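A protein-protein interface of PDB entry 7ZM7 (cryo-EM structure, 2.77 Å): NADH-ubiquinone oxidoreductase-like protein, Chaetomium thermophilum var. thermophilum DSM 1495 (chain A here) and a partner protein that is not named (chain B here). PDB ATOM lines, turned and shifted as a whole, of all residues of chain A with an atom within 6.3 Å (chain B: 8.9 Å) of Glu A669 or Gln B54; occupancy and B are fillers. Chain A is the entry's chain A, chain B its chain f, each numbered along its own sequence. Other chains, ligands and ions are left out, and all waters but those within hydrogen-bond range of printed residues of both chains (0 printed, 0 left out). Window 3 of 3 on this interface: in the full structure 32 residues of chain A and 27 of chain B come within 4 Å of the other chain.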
ATOM      1  N   ARG A 396      11.159 -19.674 -13.846  1.00  0.00           N
ATOM      2  CA  ARG A 396      11.250 -20.333 -15.173  1.00  0.00           C
ATOM      3  C   ARG A 396      11.878 -21.710 -14.995  1.00  0.00           C
ATOM      4  O   ARG A 396      11.497 -22.618 -15.738  1.00  0.00           O
ATOM      5  CB  ARG A 396      11.969 -19.465 -16.208  1.00  0.00           C
ATOM      6  CG  ARG A 396      11.140 -18.292 -16.707  1.00  0.00           C
ATOM      7  CD  ARG A 396      11.959 -17.298 -17.504  1.00  0.00           C
ATOM      8  NE  ARG A 396      12.595 -17.875 -18.676  1.00  0.00           N
ATOM      9  CZ  ARG A 396      13.903 -17.875 -18.891  1.00  0.00           C
ATOM     10  NH1 ARG A 396      14.391 -18.428 -19.989  1.00  0.00           N
ATOM     11  NH2 ARG A 396      14.718 -17.317 -18.014  1.00  0.00           N
ATOM     12  N   LEU A 400      11.381 -26.163 -16.798  1.00  0.00           N
ATOM     13  CA  LEU A 400      12.251 -26.235 -17.955  1.00  0.00           C
ATOM     14  C   LEU A 400      13.200 -27.411 -17.821  1.00  0.00           C
ATOM     15  O   LEU A 400      13.325 -28.027 -16.764  1.00  0.00           O
ATOM     16  CB  LEU A 400      13.034 -24.936 -18.147  1.00  0.00           C
ATOM     17  CG  LEU A 400      12.206 -23.841 -18.806  1.00  0.00           C
ATOM     18  CD1 LEU A 400      12.974 -22.567 -18.873  1.00  0.00           C
ATOM     19  CD2 LEU A 400      11.748 -24.261 -20.189  1.00  0.00           C
ATOM     20  N   GLY A 610      13.784 -24.046 -23.047  1.00  0.00           N
ATOM     21  CA  GLY A 610      13.611 -22.625 -22.903  1.00  0.00           C
ATOM     22  C   GLY A 610      14.161 -21.793 -24.029  1.00  0.00           C
ATOM     23  O   GLY A 610      14.308 -20.579 -23.867  1.00  0.00           O
ATOM     24  N   ARG A 611      14.482 -22.398 -25.161  1.00  0.00           N
ATOM     25  CA  ARG A 611      14.984 -21.652 -26.300  1.00  0.00           C
ATOM     26  C   ARG A 611      13.804 -21.147 -27.113  1.00  0.00           C
ATOM     27  O   ARG A 611      12.904 -21.915 -27.459  1.00  0.00           O
ATOM     28  CB  ARG A 611      15.911 -22.519 -27.143  1.00  0.00           C
ATOM     29  CG  ARG A 611      16.469 -21.857 -28.354  1.00  0.00           C
ATOM     30  CD  ARG A 611      17.432 -22.777 -29.062  1.00  0.00           C
ATOM     31  NE  ARG A 611      18.219 -23.562 -28.124  1.00  0.00           N
ATOM     32  CZ  ARG A 611      19.478 -23.294 -27.804  1.00  0.00           C
ATOM     33  NH1 ARG A 611      20.101 -22.272 -28.361  1.00  0.00           N
ATOM     34  NH2 ARG A 611      20.113 -24.058 -26.934  1.00  0.00           N
ATOM     35  N   PRO A 660      10.573 -11.109 -21.152  1.00  0.00           N
ATOM     36  CA  PRO A 660      11.534 -10.518 -22.089  1.00  0.00           C
ATOM     37  C   PRO A 660      12.359 -11.544 -22.829  1.00  0.00           C
ATOM     38  O   PRO A 660      12.880 -11.238 -23.906  1.00  0.00           O
ATOM     39  CB  PRO A 660      12.399  -9.646 -21.185  1.00  0.00           C
ATOM     40  CG  PRO A 660      12.311 -10.313 -19.868  1.00  0.00           C
ATOM     41  CD  PRO A 660      10.949 -10.866 -19.752  1.00  0.00           C
ATOM     42  N   ALA A 661      12.498 -12.746 -22.269  1.00  0.00           N
ATOM     43  CA  ALA A 661      13.225 -13.848 -22.932  1.00  0.00           C
ATOM     44  C   ALA A 661      12.574 -14.106 -24.286  1.00  0.00           C
ATOM     45  O   ALA A 661      13.289 -14.528 -25.209  1.00  0.00           O
ATOM     46  CB  ALA A 661      13.147 -15.079 -22.083  1.00  0.00           C
ATOM     47  N   LEU A 662      11.264 -13.865 -24.392  1.00  0.00           N
ATOM     48  CA  LEU A 662      10.524 -14.085 -25.660  1.00  0.00           C
ATOM     49  C   LEU A 662      11.024 -13.133 -26.743  1.00  0.00           C
ATOM     50  O   LEU A 662      10.724 -13.385 -27.916  1.00  0.00           O
ATOM     51  CB  LEU A 662       9.028 -13.923 -25.419  1.00  0.00           C
ATOM     52  CG  LEU A 662       8.367 -15.024 -24.593  1.00  0.00           C
ATOM     53  CD1 LEU A 662       6.902 -14.704 -24.355  1.00  0.00           C
ATOM     54  CD2 LEU A 662       8.509 -16.372 -25.276  1.00  0.00           C
ATOM     55  N   ALA A 664      14.351 -12.574 -27.081  1.00  0.00           N
ATOM     56  CA  ALA A 664      15.625 -13.169 -27.461  1.00  0.00           C
ATOM     57  C   ALA A 664      15.372 -14.399 -28.317  1.00  0.00           C
ATOM     58  O   ALA A 664      14.649 -15.310 -27.910  1.00  0.00           O
ATOM     59  CB  ALA A 664      16.423 -13.531 -26.217  1.00  0.00           C
ATOM     60  N   VAL A 667      18.093 -18.436 -28.582  1.00  0.00           N
ATOM     61  CA  VAL A 667      18.965 -18.517 -27.423  1.00  0.00           C
ATOM     62  C   VAL A 667      18.123 -18.893 -26.216  1.00  0.00           C
ATOM     63  O   VAL A 667      16.919 -18.629 -26.168  1.00  0.00           O
ATOM     64  CB  VAL A 667      19.729 -17.194 -27.201  1.00  0.00           C
ATOM     65  CG1 VAL A 667      18.814 -16.117 -26.683  1.00  0.00           C
ATOM     66  CG2 VAL A 667      20.910 -17.396 -26.269  1.00  0.00           C
ATOM     67  N   VAL A 668      18.759 -19.547 -25.256  1.00  0.00           N
ATOM     68  CA  VAL A 668      18.187 -19.767 -23.939  1.00  0.00           C
ATOM     69  C   VAL A 668      18.650 -18.632 -23.045  1.00  0.00           C
ATOM     70  O   VAL A 668      19.831 -18.268 -23.062  1.00  0.00           O
ATOM     71  CB  VAL A 668      18.602 -21.130 -23.358  1.00  0.00           C
ATOM     72  CG1 VAL A 668      17.935 -21.350 -22.027  1.00  0.00           C
ATOM     73  CG2 VAL A 668      18.240 -22.238 -24.298  1.00  0.00           C
ATOM     74  N   GLU A 669      17.724 -18.048 -22.296  1.00  0.00           N
ATOM     75  CA  GLU A 669      18.072 -17.079 -21.268  1.00  0.00           C
ATOM     76  C   GLU A 669      18.224 -17.797 -19.938  1.00  0.00           C
ATOM     77  O   GLU A 669      17.261 -18.420 -19.476  1.00  0.00           O
ATOM     78  CB  GLU A 669      17.009 -15.998 -21.151  1.00  0.00           C
ATOM     79  CG  GLU A 669      16.895 -15.100 -22.358  1.00  0.00           C
ATOM     80  CD  GLU A 669      17.844 -13.924 -22.305  1.00  0.00           C
ATOM     81  OE1 GLU A 669      18.910 -14.042 -21.673  1.00  0.00           O
ATOM     82  OE2 GLU A 669      17.538 -12.878 -22.908  1.00  0.00           O
ATOM     83  N   PRO A 670      19.380 -17.726 -19.287  1.00  0.00           N
ATOM     84  CA  PRO A 670      19.567 -18.468 -18.037  1.00  0.00           C
ATOM     85  C   PRO A 670      18.665 -17.941 -16.937  1.00  0.00           C
ATOM     86  O   PRO A 670      18.350 -16.753 -16.871  1.00  0.00           O
ATOM     87  CB  PRO A 670      21.042 -18.239 -17.696  1.00  0.00           C
ATOM     88  CG  PRO A 670      21.538 -17.196 -18.632  1.00  0.00           C
ATOM     89  CD  PRO A 670      20.429 -16.721 -19.499  1.00  0.00           C
ATOM     90  N   VAL A 671      18.248 -18.845 -16.069  1.00  0.00           N
ATOM     91  CA  VAL A 671      17.400 -18.496 -14.939  1.00  0.00           C
ATOM     92  C   VAL A 671      18.301 -18.039 -13.809  1.00  0.00           C
ATOM     93  O   VAL A 671      19.267 -18.723 -13.458  1.00  0.00           O
ATOM     94  CB  VAL A 671      16.522 -19.685 -14.508  1.00  0.00           C
ATOM     95  CG1 VAL A 671      15.824 -19.383 -13.203  1.00  0.00           C
ATOM     96  CG2 VAL A 671      15.500 -20.002 -15.569  1.00  0.00           C
ATOM     97  N   PHE B  18      13.450  -8.330 -15.042  1.00  0.00           N
ATOM     98  CA  PHE B  18      14.767  -7.860 -14.616  1.00  0.00           C
ATOM     99  C   PHE B  18      15.842  -8.609 -15.389  1.00  0.00           C
ATOM    100  O   PHE B  18      15.550  -9.382 -16.298  1.00  0.00           O
ATOM    101  CB  PHE B  18      14.897  -8.004 -13.100  1.00  0.00           C
ATOM    102  CG  PHE B  18      14.783  -9.398 -12.625  1.00  0.00           C
ATOM    103  CD1 PHE B  18      13.545  -9.943 -12.380  1.00  0.00           C
ATOM    104  CD2 PHE B  18      15.895 -10.145 -12.349  1.00  0.00           C
ATOM    105  CE1 PHE B  18      13.424 -11.223 -11.929  1.00  0.00           C
ATOM    106  CE2 PHE B  18      15.770 -11.424 -11.884  1.00  0.00           C
ATOM    107  CZ  PHE B  18      14.539 -11.957 -11.673  1.00  0.00           C
ATOM    108  N   CYS B  19      17.093  -8.359 -15.046  1.00  0.00           N
ATOM    109  CA  CYS B  19      18.218  -8.926 -15.763  1.00  0.00           C
ATOM    110  C   CYS B  19      19.028  -9.796 -14.813  1.00  0.00           C
ATOM    111  O   CYS B  19      19.133  -9.509 -13.622  1.00  0.00           O
ATOM    112  CB  CYS B  19      19.086  -7.835 -16.377  1.00  0.00           C
ATOM    113  SG  CYS B  19      20.469  -8.446 -17.352  1.00  0.00           S
ATOM    114  N   GLN B  20      19.589 -10.871 -15.356  1.00  0.00           N
ATOM    115  CA  GLN B  20      20.176 -11.908 -14.516  1.00  0.00           C
ATOM    116  C   GLN B  20      21.426 -11.422 -13.806  1.00  0.00           C
ATOM    117  O   GLN B  20      21.659 -11.771 -12.647  1.00  0.00           O
ATOM    118  CB  GLN B  20      20.489 -13.142 -15.356  1.00  0.00           C
ATOM    119  CG  GLN B  20      19.278 -13.778 -15.982  1.00  0.00           C
ATOM    120  CD  GLN B  20      19.047 -13.302 -17.392  1.00  0.00           C
ATOM    121  OE1 GLN B  20      19.454 -12.205 -17.756  1.00  0.00           O
ATOM    122  NE2 GLN B  20      18.388 -14.123 -18.198  1.00  0.00           N
ATOM    123  N   THR B  21      22.254 -10.643 -14.488  1.00  0.00           N
ATOM    124  CA  THR B  21      23.545 -10.262 -13.954  1.00  0.00           C
ATOM    125  C   THR B  21      23.853  -8.790 -14.127  1.00  0.00           C
ATOM    126  O   THR B  21      24.960  -8.365 -13.786  1.00  0.00           O
ATOM    127  CB  THR B  21      24.666 -11.085 -14.608  1.00  0.00           C
ATOM    128  OG1 THR B  21      25.896 -10.863 -13.908  1.00  0.00           O
ATOM    129  CG2 THR B  21      24.842 -10.682 -16.065  1.00  0.00           C
ATOM    130  N   SER B  22      22.925  -8.003 -14.654  1.00  0.00           N
ATOM    131  CA  SER B  22      23.148  -6.571 -14.748  1.00  0.00           C
ATOM    132  C   SER B  22      23.192  -5.940 -13.363  1.00  0.00           C
ATOM    133  O   SER B  22      22.563  -6.414 -12.416  1.00  0.00           O
ATOM    134  CB  SER B  22      22.059  -5.908 -15.581  1.00  0.00           C
ATOM    135  OG  SER B  22      22.104  -6.370 -16.911  1.00  0.00           O
ATOM    136  N   SER B  25      19.875  -4.517 -11.965  1.00  0.00           N
ATOM    137  CA  SER B  25      18.877  -5.450 -11.483  1.00  0.00           C
ATOM    138  C   SER B  25      19.247  -6.081 -10.156  1.00  0.00           C
ATOM    139  O   SER B  25      18.430  -6.797  -9.586  1.00  0.00           O
ATOM    140  CB  SER B  25      18.631  -6.532 -12.537  1.00  0.00           C
ATOM    141  OG  SER B  25      18.436  -5.962 -13.819  1.00  0.00           O
ATOM    142  N   ARG B  29      16.991  -7.967  -7.801  1.00  0.00           N
ATOM    143  CA  ARG B  29      17.352  -9.342  -7.492  1.00  0.00           C
ATOM    144  C   ARG B  29      17.454  -9.553  -5.992  1.00  0.00           C
ATOM    145  O   ARG B  29      17.105 -10.624  -5.482  1.00  0.00           O
ATOM    146  CB  ARG B  29      18.665  -9.710  -8.172  1.00  0.00           C
ATOM    147  CG  ARG B  29      18.569  -9.864  -9.664  1.00  0.00           C
ATOM    148  CD  ARG B  29      19.805 -10.527 -10.195  1.00  0.00           C
ATOM    149  NE  ARG B  29      21.000  -9.803  -9.797  1.00  0.00           N
ATOM    150  CZ  ARG B  29      21.664  -8.973 -10.584  1.00  0.00           C
ATOM    151  NH1 ARG B  29      22.738  -8.355 -10.131  1.00  0.00           N
ATOM    152  NH2 ARG B  29      21.263  -8.770 -11.825  1.00  0.00           N
ATOM    153  N   ARG B  51      10.283 -13.066 -14.632  1.00  0.00           N
ATOM    154  CA  ARG B  51      10.776 -13.301 -16.006  1.00  0.00           C
ATOM    155  C   ARG B  51      11.931 -12.339 -16.283  1.00  0.00           C
ATOM    156  O   ARG B  51      11.710 -11.134 -16.210  1.00  0.00           O
ATOM    157  CB  ARG B  51       9.616 -13.169 -16.996  1.00  0.00           C
ATOM    158  CG  ARG B  51       8.453 -14.115 -16.748  1.00  0.00           C
ATOM    159  CD  ARG B  51       8.810 -15.513 -17.193  1.00  0.00           C
ATOM    160  NE  ARG B  51       7.645 -16.373 -17.167  1.00  0.00           N
ATOM    161  CZ  ARG B  51       7.304 -17.149 -16.151  1.00  0.00           C
ATOM    162  NH1 ARG B  51       6.212 -17.887 -16.229  1.00  0.00           N
ATOM    163  NH2 ARG B  51       8.053 -17.188 -15.066  1.00  0.00           N
ATOM    164  N   GLU B  52      13.103 -12.866 -16.625  1.00  0.00           N
ATOM    165  CA  GLU B  52      14.296 -12.069 -16.830  1.00  0.00           C
ATOM    166  C   GLU B  52      14.856 -12.292 -18.230  1.00  0.00           C
ATOM    167  O   GLU B  52      14.376 -13.127 -18.996  1.00  0.00           O
ATOM    168  CB  GLU B  52      15.348 -12.398 -15.769  1.00  0.00           C
ATOM    169  CG  GLU B  52      15.846 -13.807 -15.844  1.00  0.00           C
ATOM    170  CD  GLU B  52      14.951 -14.786 -15.153  1.00  0.00           C
ATOM    171  OE1 GLU B  52      15.446 -15.531 -14.280  1.00  0.00           O
ATOM    172  OE2 GLU B  52      13.753 -14.815 -15.485  1.00  0.00           O
ATOM    173  N   ALA B  53      15.874 -11.508 -18.557  1.00  0.00           N
ATOM    174  CA  ALA B  53      16.572 -11.538 -19.834  1.00  0.00           C
ATOM    175  C   ALA B  53      17.726 -10.558 -19.735  1.00  0.00           C
ATOM    176  O   ALA B  53      17.673  -9.603 -18.963  1.00  0.00           O
ATOM    177  CB  ALA B  53      15.656 -11.167 -21.003  1.00  0.00           C
ATOM    178  N   GLN B  54      18.764 -10.802 -20.528  1.00  0.00           N
ATOM    179  CA  GLN B  54      19.935  -9.937 -20.525  1.00  0.00           C
ATOM    180  C   GLN B  54      19.549  -8.521 -20.905  1.00  0.00           C
ATOM    181  O   GLN B  54      18.859  -8.298 -21.900  1.00  0.00           O
ATOM    182  CB  GLN B  54      20.986 -10.460 -21.498  1.00  0.00           C
ATOM    183  CG  GLN B  54      21.314 -11.935 -21.373  1.00  0.00           C
ATOM    184  CD  GLN B  54      22.094 -12.291 -20.121  1.00  0.00           C
ATOM    185  OE1 GLN B  54      21.929 -11.681 -19.066  1.00  0.00           O
ATOM    186  NE2 GLN B  54      22.961 -13.290 -20.238  1.00  0.00           N
ATOM    187  N   GLY B  55      20.007  -7.561 -20.115  1.00  0.00           N
ATOM    188  CA  GLY B  55      19.684  -6.173 -20.367  1.00  0.00           C
ATOM    189  C   GLY B  55      18.213  -5.843 -20.243  1.00  0.00           C
ATOM    190  O   GLY B  55      17.653  -5.177 -21.116  1.00  0.00           O
ATOM    191  N   THR B  56      17.573  -6.297 -19.177  1.00  0.00           N
ATOM    192  CA  THR B  56      16.163  -6.016 -18.937  1.00  0.00           C
ATOM    193  C   THR B  56      16.066  -4.953 -17.859  1.00  0.00           C
ATOM    194  O   THR B  56      16.363  -5.222 -16.694  1.00  0.00           O
ATOM    195  CB  THR B  56      15.416  -7.278 -18.524  1.00  0.00           C
ATOM    196  OG1 THR B  56      15.796  -8.358 -19.378  1.00  0.00           O
ATOM    197  CG2 THR B  56      13.919  -7.073 -18.624  1.00  0.00           C
ATOM    198  N   ILE B  57      15.639  -3.753 -18.241  1.00  0.00           N
ATOM    199  CA  ILE B  57      15.494  -2.673 -17.257  1.00  0.00           C
ATOM    200  C   ILE B  57      14.394  -3.040 -16.272  1.00  0.00           C
ATOM    201  O   ILE B  57      13.251  -3.296 -16.693  1.00  0.00           O
ATOM    202  CB  ILE B  57      15.180  -1.346 -17.962  1.00  0.00           C
ATOM    203  CG1 ILE B  57      16.296  -0.997 -18.941  1.00  0.00           C
ATOM    204  CG2 ILE B  57      15.003  -0.235 -16.950  1.00  0.00           C
ATOM    205  CD1 ILE B  57      17.640  -0.818 -18.279  1.00  0.00           C
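No residue of chain B comes within 4 Å of Val A668. Of chain B, only Gln B20 (3.5 Å), Ala B53 (3.2 Å) and Gln B54 (3.2 Å) come within 4 Å of Glu A669. Printed residues of chain B within 4 Å of Val A671: Glu B52 (3.6 Å). Printed residues of chain A within 4 Å of Gln B20: Glu A669 and Pro A670. Ser B22 touches none of the printed residues of chain A. Gln B54 touches just one residue of chain A: Glu A669. The nearest residue of chain B that does not touch Glu A669 is Glu B52 (4.5 Å). The nearest printed residue of chain B that does not touch Arg A396 is Gln B20 (4.9 Å).
The backbone NH of Ala B53 lies within hydrogen-bond range of the backbone carbonyl oxygen of Phe B18 (3.1 Å). SG of Cys B19 lies close to O of Ala B53, 3.4 Å away. O of Gln B20 is in hydrogen-bond range of NH2 of Arg B29, at 3.1 Å. The side-chain hydroxyl (OG1) of Thr B56 lies close to the backbone carbonyl oxygen (O) of Phe B18, at 3.3 Å. The backbone NH of Ala B53 lies close to the side-chain hydroxyl of Thr B56, 3.3 Å away. OE1 of Gln B20 sits close to O of Ala B53 (3.4 Å).
CD of Arg A396 touches CD of Arg B51 (3.6 Å). CD of Pro A660 touches O of Arg B51 (3.6 Å). CG of Pro A660 touches O of Glu B52 (3.6 Å). Pro A660 touches Ala B53. Pro A660 touches Thr B56 (CG to CG2, 3.8 Å). N of Ala A661 touches O of Glu B52, 3.8 Å away. Ala A661 touches Ala B53 (N to CB, 3.8 Å). Glu A669 touches Gln B20 (OE1 to NE2, 3.5 Å). OE2 of Glu A669 touches CB of Ala B53, at 3.2 Å. Val A671 touches Glu B52.
The side-chain amide nitrogen (NE2) of Gln B20 sits at hydrogen-bond distance from the backbone carbonyl oxygen (O) of Pro A670 (2.9 Å). N of Gln B54 is in hydrogen-bond range of OE2 of Glu A669 (3.4 Å). NH2 of Arg A396 lies within salt-bridge range of OE2 of Glu B52, 3.7 Å away.
Hydrophobic or aromatic side chains of chain A within 4 Å of the printed part of chain B: Pro A660, Ala A661 and Pro A670. Among the printed residues, 13 pairs touch across the chains.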
